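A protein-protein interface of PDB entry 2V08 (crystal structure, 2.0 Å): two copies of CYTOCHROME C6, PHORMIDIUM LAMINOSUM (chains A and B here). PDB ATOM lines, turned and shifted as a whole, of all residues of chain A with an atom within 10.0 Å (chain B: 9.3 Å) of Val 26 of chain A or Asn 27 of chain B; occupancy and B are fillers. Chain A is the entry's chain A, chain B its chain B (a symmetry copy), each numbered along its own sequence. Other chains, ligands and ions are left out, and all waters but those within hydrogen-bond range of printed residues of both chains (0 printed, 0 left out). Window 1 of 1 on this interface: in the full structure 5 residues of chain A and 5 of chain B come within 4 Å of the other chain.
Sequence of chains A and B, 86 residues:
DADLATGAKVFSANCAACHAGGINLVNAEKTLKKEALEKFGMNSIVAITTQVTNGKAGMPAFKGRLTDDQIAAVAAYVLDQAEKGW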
ATOM      1  N   CYS A  15      -4.476 -26.399 -16.329  1.00  0.00           N
ATOM      2  CA  CYS A  15      -5.577 -26.450 -17.326  1.00  0.00           C
ATOM      3  C   CYS A  15      -6.101 -27.866 -17.542  1.00  0.00           C
ATOM      4  O   CYS A  15      -7.254 -28.036 -17.906  1.00  0.00           O
ATOM      5  CB  CYS A  15      -5.110 -25.970 -18.677  1.00  0.00           C
ATOM      6  SG  CYS A  15      -4.059 -24.439 -18.688  1.00  0.00           S
ATOM      7  N   ALA A  16      -5.249 -28.844 -17.253  1.00  0.00           N
ATOM      8  CA  ALA A  16      -5.584 -30.256 -17.484  1.00  0.00           C
ATOM      9  C   ALA A  16      -6.759 -30.742 -16.611  1.00  0.00           C
ATOM     10  O   ALA A  16      -7.468 -31.647 -17.045  1.00  0.00           O
ATOM     11  CB  ALA A  16      -4.348 -31.156 -17.340  1.00  0.00           C
ATOM     12  N   ALA A  17      -6.988 -30.133 -15.435  1.00  0.00           N
ATOM     13  CA  ALA A  17      -8.119 -30.499 -14.551  1.00  0.00           C
ATOM     14  C   ALA A  17      -9.442 -30.439 -15.368  1.00  0.00           C
ATOM     15  O   ALA A  17     -10.272 -31.369 -15.336  1.00  0.00           O
ATOM     16  CB  ALA A  17      -8.187 -29.565 -13.305  1.00  0.00           C
ATOM     17  N   CYS A  18      -9.591 -29.403 -16.177  1.00  0.00           N
ATOM     18  CA  CYS A  18     -10.865 -29.223 -16.943  1.00  0.00           C
ATOM     19  C   CYS A  18     -10.718 -29.488 -18.423  1.00  0.00           C
ATOM     20  O   CYS A  18     -11.707 -29.642 -19.113  1.00  0.00           O
ATOM     21  CB  CYS A  18     -11.331 -27.781 -16.826  1.00  0.00           C
ATOM     22  SG  CYS A  18     -11.688 -27.342 -15.141  1.00  0.00           S
ATOM     23  N   HIS A  19      -9.498 -29.467 -18.924  1.00  0.00           N
ATOM     24  CA  HIS A  19      -9.296 -29.656 -20.372  1.00  0.00           C
ATOM     25  C   HIS A  19      -8.394 -30.825 -20.761  1.00  0.00           C
ATOM     26  O   HIS A  19      -7.777 -30.777 -21.811  1.00  0.00           O
ATOM     27  CB  HIS A  19      -8.667 -28.393 -21.009  1.00  0.00           C
ATOM     28  CG  HIS A  19      -9.540 -27.172 -20.951  1.00  0.00           C
ATOM     29  ND1 HIS A  19     -10.707 -27.046 -21.668  1.00  0.00           N
ATOM     30  CD2 HIS A  19      -9.387 -26.003 -20.275  1.00  0.00           C
ATOM     31  CE1 HIS A  19     -11.240 -25.849 -21.442  1.00  0.00           C
ATOM     32  NE2 HIS A  19     -10.436 -25.192 -20.622  1.00  0.00           N
ATOM     33  N   ALA A  20      -8.343 -31.864 -19.948  1.00  0.00           N
ATOM     34  CA  ALA A  20      -7.364 -32.936 -20.177  1.00  0.00           C
ATOM     35  C   ALA A  20      -7.533 -33.500 -21.564  1.00  0.00           C
ATOM     36  O   ALA A  20      -8.635 -33.891 -21.968  1.00  0.00           O
ATOM     37  CB  ALA A  20      -7.534 -34.063 -19.149  1.00  0.00           C
ATOM     38  N   GLY A  22      -7.591 -32.008 -24.342  1.00  0.00           N
ATOM     39  CA  GLY A  22      -8.312 -31.131 -25.278  1.00  0.00           C
ATOM     40  C   GLY A  22      -9.822 -31.066 -25.073  1.00  0.00           C
ATOM     41  O   GLY A  22     -10.546 -30.382 -25.844  1.00  0.00           O
ATOM     42  N   ILE A  23     -10.319 -31.736 -24.034  1.00  0.00           N
ATOM     43  CA  ILE A  23     -11.763 -31.705 -23.747  1.00  0.00           C
ATOM     44  C   ILE A  23     -12.180 -30.431 -23.004  1.00  0.00           C
ATOM     45  O   ILE A  23     -11.340 -29.569 -22.692  1.00  0.00           O
ATOM     46  CB  ILE A  23     -12.187 -32.892 -22.841  1.00  0.00           C
ATOM     47  CG1 ILE A  23     -11.664 -32.700 -21.397  1.00  0.00           C
ATOM     48  CG2 ILE A  23     -11.794 -34.236 -23.480  1.00  0.00           C
ATOM     49  CD1 ILE A  23     -11.978 -33.883 -20.440  1.00  0.00           C
ATOM     50  N   ASN A  24     -13.475 -30.320 -22.696  1.00  0.00           N
ATOM     51  CA  ASN A  24     -13.961 -29.299 -21.752  1.00  0.00           C
ATOM     52  C   ASN A  24     -14.999 -29.957 -20.844  1.00  0.00           C
ATOM     53  O   ASN A  24     -16.140 -30.220 -21.251  1.00  0.00           O
ATOM     54  CB  ASN A  24     -14.521 -28.061 -22.463  1.00  0.00           C
ATOM     55  CG  ASN A  24     -14.844 -26.921 -21.502  1.00  0.00           C
ATOM     56  OD1 ASN A  24     -15.179 -27.156 -20.338  1.00  0.00           O
ATOM     57  ND2 ASN A  24     -14.767 -25.667 -21.994  1.00  0.00           N
ATOM     58  N   LEU A  25     -14.574 -30.207 -19.608  1.00  0.00           N
ATOM     59  CA  LEU A  25     -15.354 -30.979 -18.629  1.00  0.00           C
ATOM     60  C   LEU A  25     -16.541 -30.172 -18.159  1.00  0.00           C
ATOM     61  O   LEU A  25     -17.529 -30.743 -17.700  1.00  0.00           O
ATOM     62  CB  LEU A  25     -14.494 -31.247 -17.380  1.00  0.00           C
ATOM     63  CG  LEU A  25     -13.632 -32.477 -17.326  1.00  0.00           C
ATOM     64  CD1 LEU A  25     -12.987 -32.609 -15.975  1.00  0.00           C
ATOM     65  CD2 LEU A  25     -14.511 -33.658 -17.609  1.00  0.00           C
ATOM     66  N   VAL A  26     -16.421 -28.846 -18.238  1.00  0.00           N
ATOM     67  CA  VAL A  26     -17.411 -27.934 -17.631  1.00  0.00           C
ATOM     68  C   VAL A  26     -18.489 -27.497 -18.626  1.00  0.00           C
ATOM     69  O   VAL A  26     -19.664 -27.560 -18.336  1.00  0.00           O
ATOM     70  CB  VAL A  26     -16.691 -26.702 -16.934  1.00  0.00           C
ATOM     71  CG1 VAL A  26     -17.708 -25.722 -16.286  1.00  0.00           C
ATOM     72  CG2 VAL A  26     -15.749 -27.234 -15.892  1.00  0.00           C
ATOM     73  N   ASN A  27     -18.062 -27.150 -19.831  1.00  0.00           N
ATOM     74  CA  ASN A  27     -18.960 -26.727 -20.876  1.00  0.00           C
ATOM     75  C   ASN A  27     -18.603 -27.511 -22.106  1.00  0.00           C
ATOM     76  O   ASN A  27     -17.640 -27.192 -22.830  1.00  0.00           O
ATOM     77  CB  ASN A  27     -18.898 -25.198 -21.026  1.00  0.00           C
ATOM     78  CG  ASN A  27     -19.931 -24.695 -21.969  1.00  0.00           C
ATOM     79  OD1 ASN A  27     -20.409 -25.481 -22.776  1.00  0.00           O
ATOM     80  ND2 ASN A  27     -20.226 -23.378 -21.952  1.00  0.00           N
ATOM     81  N   ALA A  28     -19.310 -28.636 -22.285  1.00  0.00           N
ATOM     82  CA  ALA A  28     -18.809 -29.717 -23.160  1.00  0.00           C
ATOM     83  C   ALA A  28     -18.462 -29.319 -24.588  1.00  0.00           C
ATOM     84  O   ALA A  28     -17.530 -29.851 -25.126  1.00  0.00           O
ATOM     85  CB  ALA A  28     -19.777 -30.921 -23.201  1.00  0.00           C
ATOM     86  N   GLU A  29     -19.228 -28.427 -25.207  1.00  0.00           N
ATOM     87  CA  GLU A  29     -18.946 -28.084 -26.623  1.00  0.00           C
ATOM     88  C   GLU A  29     -17.721 -27.204 -26.816  1.00  0.00           C
ATOM     89  O   GLU A  29     -17.138 -27.185 -27.915  1.00  0.00           O
ATOM     90  CB  GLU A  29     -20.123 -27.375 -27.306  1.00  0.00           C
ATOM     91  CG  GLU A  29     -21.456 -28.037 -27.125  1.00  0.00           C
ATOM     92  CD  GLU A  29     -22.243 -27.371 -25.986  1.00  0.00           C
ATOM     93  OE1 GLU A  29     -21.674 -27.093 -24.863  1.00  0.00           O
ATOM     94  OE2 GLU A  29     -23.426 -27.090 -26.234  1.00  0.00           O
ATOM     95  N   LYS A  30     -17.333 -26.478 -25.776  1.00  0.00           N
ATOM     96  CA  LYS A  30     -16.161 -25.554 -25.877  1.00  0.00           C
ATOM     97  C   LYS A  30     -14.787 -26.204 -25.624  1.00  0.00           C
ATOM     98  O   LYS A  30     -13.998 -25.798 -24.705  1.00  0.00           O
ATOM     99  CB  LYS A  30     -16.431 -24.341 -24.948  1.00  0.00           C
ATOM    100  CG  LYS A  30     -17.326 -23.325 -25.686  1.00  0.00           C
ATOM    101  CD  LYS A  30     -18.168 -22.493 -24.759  1.00  0.00           C
ATOM    102  CE  LYS A  30     -18.947 -21.448 -25.587  1.00  0.00           C
ATOM    103  NZ  LYS A  30     -19.238 -20.299 -24.768  1.00  0.00           N
ATOM    104  N   THR A  31     -14.503 -27.222 -26.436  1.00  0.00           N
ATOM    105  CA  THR A  31     -13.263 -28.012 -26.392  1.00  0.00           C
ATOM    106  C   THR A  31     -12.061 -27.184 -26.928  1.00  0.00           C
ATOM    107  O   THR A  31     -12.223 -26.041 -27.426  1.00  0.00           O
ATOM    108  CB  THR A  31     -13.398 -29.317 -27.254  1.00  0.00           C
ATOM    109  OG1 THR A  31     -13.246 -28.970 -28.638  1.00  0.00           O
ATOM    110  CG2 THR A  31     -14.783 -30.006 -27.021  1.00  0.00           C
ATOM    111  N   LYS A  56     -13.910 -16.532 -18.360  1.00  0.00           N
ATOM    112  CA  LYS A  56     -15.227 -16.387 -18.937  1.00  0.00           C
ATOM    113  C   LYS A  56     -16.111 -17.483 -18.338  1.00  0.00           C
ATOM    114  O   LYS A  56     -15.757 -18.663 -18.378  1.00  0.00           O
ATOM    115  CB  LYS A  56     -15.171 -16.441 -20.462  1.00  0.00           C
ATOM    116  CG  LYS A  56     -16.537 -16.160 -21.077  1.00  0.00           C
ATOM    117  CD  LYS A  56     -16.483 -16.019 -22.519  1.00  0.00           C
ATOM    118  CE  LYS A  56     -17.869 -16.415 -23.085  1.00  0.00           C
ATOM    119  NZ  LYS A  56     -17.958 -16.123 -24.549  1.00  0.00           N
ATOM    120  N   ALA A  57     -17.199 -17.070 -17.689  1.00  0.00           N
ATOM    121  CA  ALA A  57     -18.154 -17.991 -17.069  1.00  0.00           C
ATOM    122  C   ALA A  57     -17.414 -18.985 -16.133  1.00  0.00           C
ATOM    123  O   ALA A  57     -16.666 -18.564 -15.236  1.00  0.00           O
ATOM    124  CB  ALA A  57     -19.005 -18.686 -18.188  1.00  0.00           C
ATOM    125  N   GLY A  58     -17.544 -20.290 -16.357  1.00  0.00           N
ATOM    126  CA  GLY A  58     -16.821 -21.238 -15.503  1.00  0.00           C
ATOM    127  C   GLY A  58     -15.307 -21.341 -15.694  1.00  0.00           C
ATOM    128  O   GLY A  58     -14.625 -22.083 -14.987  1.00  0.00           O
ATOM    129  N   MET A  59     -14.784 -20.672 -16.692  1.00  0.00           N
ATOM    130  CA  MET A  59     -13.363 -20.670 -16.827  1.00  0.00           C
ATOM    131  C   MET A  59     -12.758 -19.568 -15.986  1.00  0.00           C
ATOM    132  O   MET A  59     -13.131 -18.409 -16.175  1.00  0.00           O
ATOM    133  CB  MET A  59     -12.900 -20.490 -18.243  1.00  0.00           C
ATOM    134  CG  MET A  59     -11.392 -20.466 -18.134  1.00  0.00           C
ATOM    135  SD  MET A  59     -10.713 -20.799 -19.643  1.00  0.00           S
ATOM    136  CE  MET A  59      -9.077 -20.003 -19.543  1.00  0.00           C
ATOM    137  N   PRO A  60     -11.833 -19.932 -15.055  1.00  0.00           N
ATOM    138  CA  PRO A  60     -11.161 -18.945 -14.205  1.00  0.00           C
ATOM    139  C   PRO A  60     -10.284 -17.916 -14.958  1.00  0.00           C
ATOM    140  O   PRO A  60      -9.738 -18.144 -16.041  1.00  0.00           O
ATOM    141  CB  PRO A  60     -10.308 -19.796 -13.243  1.00  0.00           C
ATOM    142  CG  PRO A  60     -10.823 -21.242 -13.387  1.00  0.00           C
ATOM    143  CD  PRO A  60     -11.350 -21.312 -14.798  1.00  0.00           C
ATOM    144  N   CYS B  18     -29.772 -35.256 -20.284  1.00  0.00           N
ATOM    145  CA  CYS B  18     -28.862 -34.169 -19.874  1.00  0.00           C
ATOM    146  C   CYS B  18     -29.020 -33.716 -18.451  1.00  0.00           C
ATOM    147  O   CYS B  18     -28.099 -33.165 -17.834  1.00  0.00           O
ATOM    148  CB  CYS B  18     -29.029 -32.963 -20.797  1.00  0.00           C
ATOM    149  SG  CYS B  18     -28.665 -33.364 -22.511  1.00  0.00           S
ATOM    150  N   HIS B  19     -30.188 -33.961 -17.898  1.00  0.00           N
ATOM    151  CA  HIS B  19     -30.444 -33.457 -16.562  1.00  0.00           C
ATOM    152  C   HIS B  19     -30.826 -34.525 -15.614  1.00  0.00           C
ATOM    153  O   HIS B  19     -31.545 -34.262 -14.704  1.00  0.00           O
ATOM    154  CB  HIS B  19     -31.570 -32.440 -16.590  1.00  0.00           C
ATOM    155  CG  HIS B  19     -31.313 -31.249 -17.465  1.00  0.00           C
ATOM    156  ND1 HIS B  19     -30.421 -30.253 -17.129  1.00  0.00           N
ATOM    157  CD2 HIS B  19     -31.902 -30.859 -18.620  1.00  0.00           C
ATOM    158  CE1 HIS B  19     -30.453 -29.306 -18.053  1.00  0.00           C
ATOM    159  NE2 HIS B  19     -31.378 -29.636 -18.949  1.00  0.00           N
ATOM    160  N   GLY B  22     -31.459 -33.887 -11.740  1.00  0.00           N
ATOM    161  CA  GLY B  22     -31.264 -32.439 -11.513  1.00  0.00           C
ATOM    162  C   GLY B  22     -29.904 -31.848 -11.864  1.00  0.00           C
ATOM    163  O   GLY B  22     -29.662 -30.672 -11.580  1.00  0.00           O
ATOM    164  N   ILE B  23     -29.007 -32.632 -12.493  1.00  0.00           N
ATOM    165  CA  ILE B  23     -27.679 -32.120 -12.873  1.00  0.00           C
ATOM    166  C   ILE B  23     -27.744 -31.433 -14.230  1.00  0.00           C
ATOM    167  O   ILE B  23     -28.798 -31.347 -14.850  1.00  0.00           O
ATOM    168  CB  ILE B  23     -26.647 -33.261 -13.044  1.00  0.00           C
ATOM    169  CG1 ILE B  23     -26.877 -33.980 -14.403  1.00  0.00           C
ATOM    170  CG2 ILE B  23     -26.709 -34.194 -11.852  1.00  0.00           C
ATOM    171  CD1 ILE B  23     -26.421 -35.421 -14.508  1.00  0.00           C
ATOM    172  N   ASN B  24     -26.595 -31.005 -14.743  1.00  0.00           N
ATOM    173  CA  ASN B  24     -26.532 -30.618 -16.158  1.00  0.00           C
ATOM    174  C   ASN B  24     -25.210 -31.149 -16.726  1.00  0.00           C
ATOM    175  O   ASN B  24     -24.134 -30.590 -16.432  1.00  0.00           O
ATOM    176  CB  ASN B  24     -26.605 -29.106 -16.265  1.00  0.00           C
ATOM    177  CG  ASN B  24     -26.694 -28.598 -17.674  1.00  0.00           C
ATOM    178  OD1 ASN B  24     -26.098 -29.120 -18.614  1.00  0.00           O
ATOM    179  ND2 ASN B  24     -27.400 -27.481 -17.825  1.00  0.00           N
ATOM    180  N   LEU B  25     -25.302 -32.200 -17.558  1.00  0.00           N
ATOM    181  CA  LEU B  25     -24.088 -32.895 -18.065  1.00  0.00           C
ATOM    182  C   LEU B  25     -23.342 -32.059 -19.065  1.00  0.00           C
ATOM    183  O   LEU B  25     -22.146 -32.297 -19.323  1.00  0.00           O
ATOM    184  CB  LEU B  25     -24.489 -34.219 -18.765  1.00  0.00           C
ATOM    185  CG  LEU B  25     -24.918 -35.370 -17.904  1.00  0.00           C
ATOM    186  CD1 LEU B  25     -25.386 -36.524 -18.798  1.00  0.00           C
ATOM    187  CD2 LEU B  25     -23.736 -35.776 -17.088  1.00  0.00           C
ATOM    188  N   VAL B  26     -24.062 -31.092 -19.653  1.00  0.00           N
ATOM    189  CA  VAL B  26     -23.514 -30.292 -20.769  1.00  0.00           C
ATOM    190  C   VAL B  26     -22.838 -28.999 -20.254  1.00  0.00           C
ATOM    191  O   VAL B  26     -21.734 -28.693 -20.632  1.00  0.00           O
ATOM    192  CB  VAL B  26     -24.577 -30.022 -21.842  1.00  0.00           C
ATOM    193  CG1 VAL B  26     -24.010 -29.258 -23.051  1.00  0.00           C
ATOM    194  CG2 VAL B  26     -25.206 -31.364 -22.338  1.00  0.00           C
ATOM    195  N   ASN B  27     -23.485 -28.283 -19.344  1.00  0.00           N
ATOM    196  CA  ASN B  27     -22.904 -27.027 -18.816  1.00  0.00           C
ATOM    197  C   ASN B  27     -23.033 -27.132 -17.303  1.00  0.00           C
ATOM    198  O   ASN B  27     -24.065 -26.839 -16.746  1.00  0.00           O
ATOM    199  CB  ASN B  27     -23.606 -25.789 -19.453  1.00  0.00           C
ATOM    200  CG  ASN B  27     -22.934 -24.470 -19.078  1.00  0.00           C
ATOM    201  OD1 ASN B  27     -22.250 -24.391 -18.057  1.00  0.00           O
ATOM    202  ND2 ASN B  27     -23.178 -23.413 -19.862  1.00  0.00           N
ATOM    203  N   ALA B  28     -22.006 -27.674 -16.658  1.00  0.00           N
ATOM    204  CA  ALA B  28     -22.122 -28.227 -15.314  1.00  0.00           C
ATOM    205  C   ALA B  28     -22.820 -27.342 -14.265  1.00  0.00           C
ATOM    206  O   ALA B  28     -23.570 -27.862 -13.467  1.00  0.00           O
ATOM    207  CB  ALA B  28     -20.765 -28.661 -14.801  1.00  0.00           C
ATOM    208  N   GLU B  29     -22.559 -26.028 -14.262  1.00  0.00           N
ATOM    209  CA  GLU B  29     -23.112 -25.161 -13.201  1.00  0.00           C
ATOM    210  C   GLU B  29     -24.613 -24.848 -13.367  1.00  0.00           C
ATOM    211  O   GLU B  29     -25.285 -24.403 -12.416  1.00  0.00           O
ATOM    212  CB  GLU B  29     -22.339 -23.852 -13.118  1.00  0.00           C
ATOM    213  CG  GLU B  29     -20.836 -24.058 -13.139  1.00  0.00           C
ATOM    214  CD  GLU B  29     -20.091 -22.825 -13.550  1.00  0.00           C
ATOM    215  OE1 GLU B  29     -19.532 -22.855 -14.653  1.00  0.00           O
ATOM    216  OE2 GLU B  29     -20.057 -21.815 -12.772  1.00  0.00           O
ATOM    217  N   LYS B  30     -25.138 -25.089 -14.558  1.00  0.00           N
ATOM    218  CA  LYS B  30     -26.500 -24.718 -14.864  1.00  0.00           C
ATOM    219  C   LYS B  30     -27.469 -25.854 -14.579  1.00  0.00           C
ATOM    220  O   LYS B  30     -28.231 -26.290 -15.444  1.00  0.00           O
ATOM    221  CB  LYS B  30     -26.578 -24.165 -16.283  1.00  0.00           C
ATOM    222  CG  LYS B  30     -26.073 -22.732 -16.310  1.00  0.00           C
ATOM    223  CD  LYS B  30     -26.404 -21.984 -17.589  1.00  0.00           C
ATOM    224  CE  LYS B  30     -25.762 -20.551 -17.604  1.00  0.00           C
ATOM    225  NZ  LYS B  30     -25.939 -19.914 -18.954  1.00  0.00           N
ATOM    226  N   THR B  31     -27.417 -26.310 -13.331  1.00  0.00           N
ATOM    227  CA  THR B  31     -28.178 -27.448 -12.851  1.00  0.00           C
ATOM    228  C   THR B  31     -29.662 -27.081 -12.722  1.00  0.00           C
ATOM    229  O   THR B  31     -30.063 -25.947 -12.946  1.00  0.00           O
ATOM    230  CB  THR B  31     -27.613 -27.991 -11.497  1.00  0.00           C
ATOM    231  OG1 THR B  31     -28.087 -27.176 -10.408  1.00  0.00           O
ATOM    232  CG2 THR B  31     -26.083 -27.964 -11.481  1.00  0.00           C
ATOM    233  N   LEU B  32     -30.467 -28.065 -12.369  1.00  0.00           N
ATOM    234  CA  LEU B  32     -31.886 -27.852 -12.090  1.00  0.00           C
ATOM    235  C   LEU B  32     -32.171 -27.763 -10.572  1.00  0.00           C
ATOM    236  O   LEU B  32     -33.319 -27.843 -10.130  1.00  0.00           O
ATOM    237  CB  LEU B  32     -32.702 -28.989 -12.724  1.00  0.00           C
ATOM    238  CG  LEU B  32     -32.521 -29.198 -14.234  1.00  0.00           C
ATOM    239  CD1 LEU B  32     -33.680 -29.996 -14.803  1.00  0.00           C
ATOM    240  CD2 LEU B  32     -32.391 -27.937 -15.015  1.00  0.00           C
ATOM    241  N   ALA B  36     -29.497 -23.318  -7.849  1.00  0.00           N
ATOM    242  CA  ALA B  36     -28.982 -22.925  -9.180  1.00  0.00           C
ATOM    243  C   ALA B  36     -30.037 -22.205  -9.993  1.00  0.00           C
ATOM    244  O   ALA B  36     -29.755 -21.204 -10.641  1.00  0.00           O
ATOM    245  CB  ALA B  36     -28.446 -24.126  -9.954  1.00  0.00           C
ATOM    246  N   PHE B  40     -29.381 -18.321 -11.525  1.00  0.00           N
ATOM    247  CA  PHE B  40     -29.455 -17.914 -12.936  1.00  0.00           C
ATOM    248  C   PHE B  40     -30.824 -17.337 -13.320  1.00  0.00           C
ATOM    249  O   PHE B  40     -31.057 -17.050 -14.502  1.00  0.00           O
ATOM    250  CB  PHE B  40     -29.103 -19.069 -13.890  1.00  0.00           C
ATOM    251  CG  PHE B  40     -27.727 -19.614 -13.694  1.00  0.00           C
ATOM    252  CD1 PHE B  40     -26.614 -18.930 -14.174  1.00  0.00           C
ATOM    253  CD2 PHE B  40     -27.532 -20.801 -12.997  1.00  0.00           C
ATOM    254  CE1 PHE B  40     -25.345 -19.434 -13.982  1.00  0.00           C
ATOM    255  CE2 PHE B  40     -26.279 -21.297 -12.801  1.00  0.00           C
ATOM    256  CZ  PHE B  40     -25.168 -20.617 -13.292  1.00  0.00           C
ATOM    257  N   GLN B  51     -37.321 -21.072 -22.134  1.00  0.00           N
ATOM    258  CA  GLN B  51     -36.068 -21.721 -22.507  1.00  0.00           C
ATOM    259  C   GLN B  51     -36.332 -23.043 -23.180  1.00  0.00           C
ATOM    260  O   GLN B  51     -35.710 -23.357 -24.188  1.00  0.00           O
ATOM    261  CB  GLN B  51     -35.148 -21.939 -21.312  1.00  0.00           C
ATOM    262  CG  GLN B  51     -33.712 -22.342 -21.764  1.00  0.00           C
ATOM    263  CD  GLN B  51     -32.652 -21.892 -20.789  1.00  0.00           C
ATOM    264  OE1 GLN B  51     -32.445 -20.694 -20.589  1.00  0.00           O
ATOM    265  NE2 GLN B  51     -31.964 -22.849 -20.180  1.00  0.00           N
ATOM    266  N   LYS B  56     -31.392 -22.706 -25.870  1.00  0.00           N
ATOM    267  CA  LYS B  56     -30.365 -21.759 -25.443  1.00  0.00           C
ATOM    268  C   LYS B  56     -29.025 -22.511 -25.404  1.00  0.00           C
ATOM    269  O   LYS B  56     -28.885 -23.502 -24.678  1.00  0.00           O
ATOM    270  CB  LYS B  56     -30.707 -21.221 -24.045  1.00  0.00           C
ATOM    271  CG  LYS B  56     -29.568 -20.573 -23.295  1.00  0.00           C
ATOM    272  CD  LYS B  56     -29.582 -19.065 -23.433  1.00  0.00           C
ATOM    273  CE  LYS B  56     -28.792 -18.401 -22.331  1.00  0.00           C
ATOM    274  NZ  LYS B  56     -29.407 -18.653 -20.975  1.00  0.00           N
ATOM    275  N   ALA B  57     -28.059 -22.059 -26.186  1.00  0.00           N
ATOM    276  CA  ALA B  57     -26.772 -22.736 -26.264  1.00  0.00           C
ATOM    277  C   ALA B  57     -27.009 -24.242 -26.486  1.00  0.00           C
ATOM    278  O   ALA B  57     -27.748 -24.594 -27.393  1.00  0.00           O
ATOM    279  CB  ALA B  57     -25.879 -22.429 -25.010  1.00  0.00           C
ATOM    280  N   GLY B  58     -26.445 -25.116 -25.646  1.00  0.00           N
ATOM    281  CA  GLY B  58     -26.512 -26.573 -25.888  1.00  0.00           C
ATOM    282  C   GLY B  58     -27.881 -27.186 -25.607  1.00  0.00           C
ATOM    283  O   GLY B  58     -28.124 -28.352 -25.913  1.00  0.00           O
ATOM    284  N   MET B  59     -28.777 -26.402 -25.018  1.00  0.00           N
ATOM    285  CA  MET B  59     -30.102 -26.890 -24.745  1.00  0.00           C
ATOM    286  C   MET B  59     -30.993 -26.755 -25.974  1.00  0.00           C
ATOM    287  O   MET B  59     -31.198 -25.636 -26.463  1.00  0.00           O
ATOM    288  CB  MET B  59     -30.749 -26.144 -23.596  1.00  0.00           C
ATOM    289  CG  MET B  59     -32.196 -26.523 -23.491  1.00  0.00           C
ATOM    290  SD  MET B  59     -32.652 -26.669 -21.830  1.00  0.00           S
ATOM    291  CE  MET B  59     -34.476 -26.707 -21.924  1.00  0.00           C
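The backbone carbonyl oxygen (O) of Val 26 of chain A sits at hydrogen-bond distance from the backbone NH (N) of Ala 28 of chain B (2.9 Å). O of Val 26 of chain B sits at hydrogen-bond distance from N of Ala 28 of chain A (2.9 Å). O of Val 26 of chain A sits close to O of Val 26 of chain B (3.3 Å).
The backbone NH (N) of Val 26 of chain A is in hydrogen-bond range of the side-chain amide oxygen (OD1) of Asn 24 of chain A, 3.0 Å away. The side-chain amide oxygen (OD1) of Asn 24 of chain A is in hydrogen-bond range of the backbone NH (N) of Asn 27 of chain A, 2.9 Å away. The backbone NH (N) of Val 26 of chain B lies within hydrogen-bond range of the side-chain amide oxygen (OD1) of Asn 24 of chain B. The side-chain amide oxygen (OD1) of Asn 24 of chain B lies within hydrogen-bond range of the backbone NH (N) of Asn 27 of chain B.
O of Val 26 of chain A touches CA of Asn 27 of chain B, 3.3 Å away. OE1 of Glu 29 of chain B touches CG1 of Val 26 of chain A, at 3.8 Å. Asn 27 of chain A touches Val 26 of chain B (CA to O, 3.4 Å). ND2 of Asn 27 of chain A touches ND2 of Asn 27 of chain B, 3.6 Å away. OE1 of Glu 29 of chain A touches CG1 of Val 26 of chain B, 3.7 Å away. Glu 29 of chain A touches Gly 58 of chain B (OE2 to CA, 3.1 Å). Gly 58 of chain A touches Glu 29 of chain B.
Of chain B, only Val 26 (3.3 Å), Asn 27 (3.3 Å), Ala 28 (2.9 Å) and Glu 29 (3.8 Å) come within 4 Å of Val 26 of chain A. Printed residues of chain B within 4 Å of Glu 29 of chain A: Val 26 (3.7 Å) and Gly 58 (3.1 Å). Lys 56 of chain A touches none of the printed residues of chain B. Of the printed residues of chain B, Gly 58 of chain A touches Glu 29. Asn 27 of chain B touches just these residues of chain A: Val 26 and Asn 27. Ala 28 of chain B touches one residue of chain A. Of chain A, only Val 26 (3.8 Å) and Gly 58 (3.3 Å) come within 4 Å of Glu 29 of chain B. Lys 30 of chain B touches none of the printed residues of chain A. Met 59 of chain B touches none of the printed residues of chain A. The nearest residue of chain B that does not touch Val 26 of chain A is Leu 25 of chain B (5.4 Å). The nearest residue of chain A that does not touch Asn 27 of chain B is Ala 28 of chain A (5.1 Å).
Hydrophobic or aromatic side chains of chain A that line the printed part of chain B: Val 26 and Ala 28. Printed residues of chain B that touch a printed residue of chain A: Val 26, Asn 27, Ala 28, Glu 29 and Gly 58. Among the printed residues, no Asp or Glu carboxylate lies within 4 Å of a Lys or Arg side-chain nitrogen of the other chain.
Val 26 of chain B touches its own counterpart, Val 26 of chain A. Val 26 of chain A touches Asn 27 of chain B, and with the chains exchanged Asn 27 of chain A touches Val 26 of chain B. Val 26 of chain A touches Ala 28 of chain B, and with the chains exchanged Ala 28 of chain A touches Val 26 of chain B. Glu 29 of chain A touches Gly 58 of chain B, and with the chains exchanged Gly 58 of chain A touches Glu 29 of chain B.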
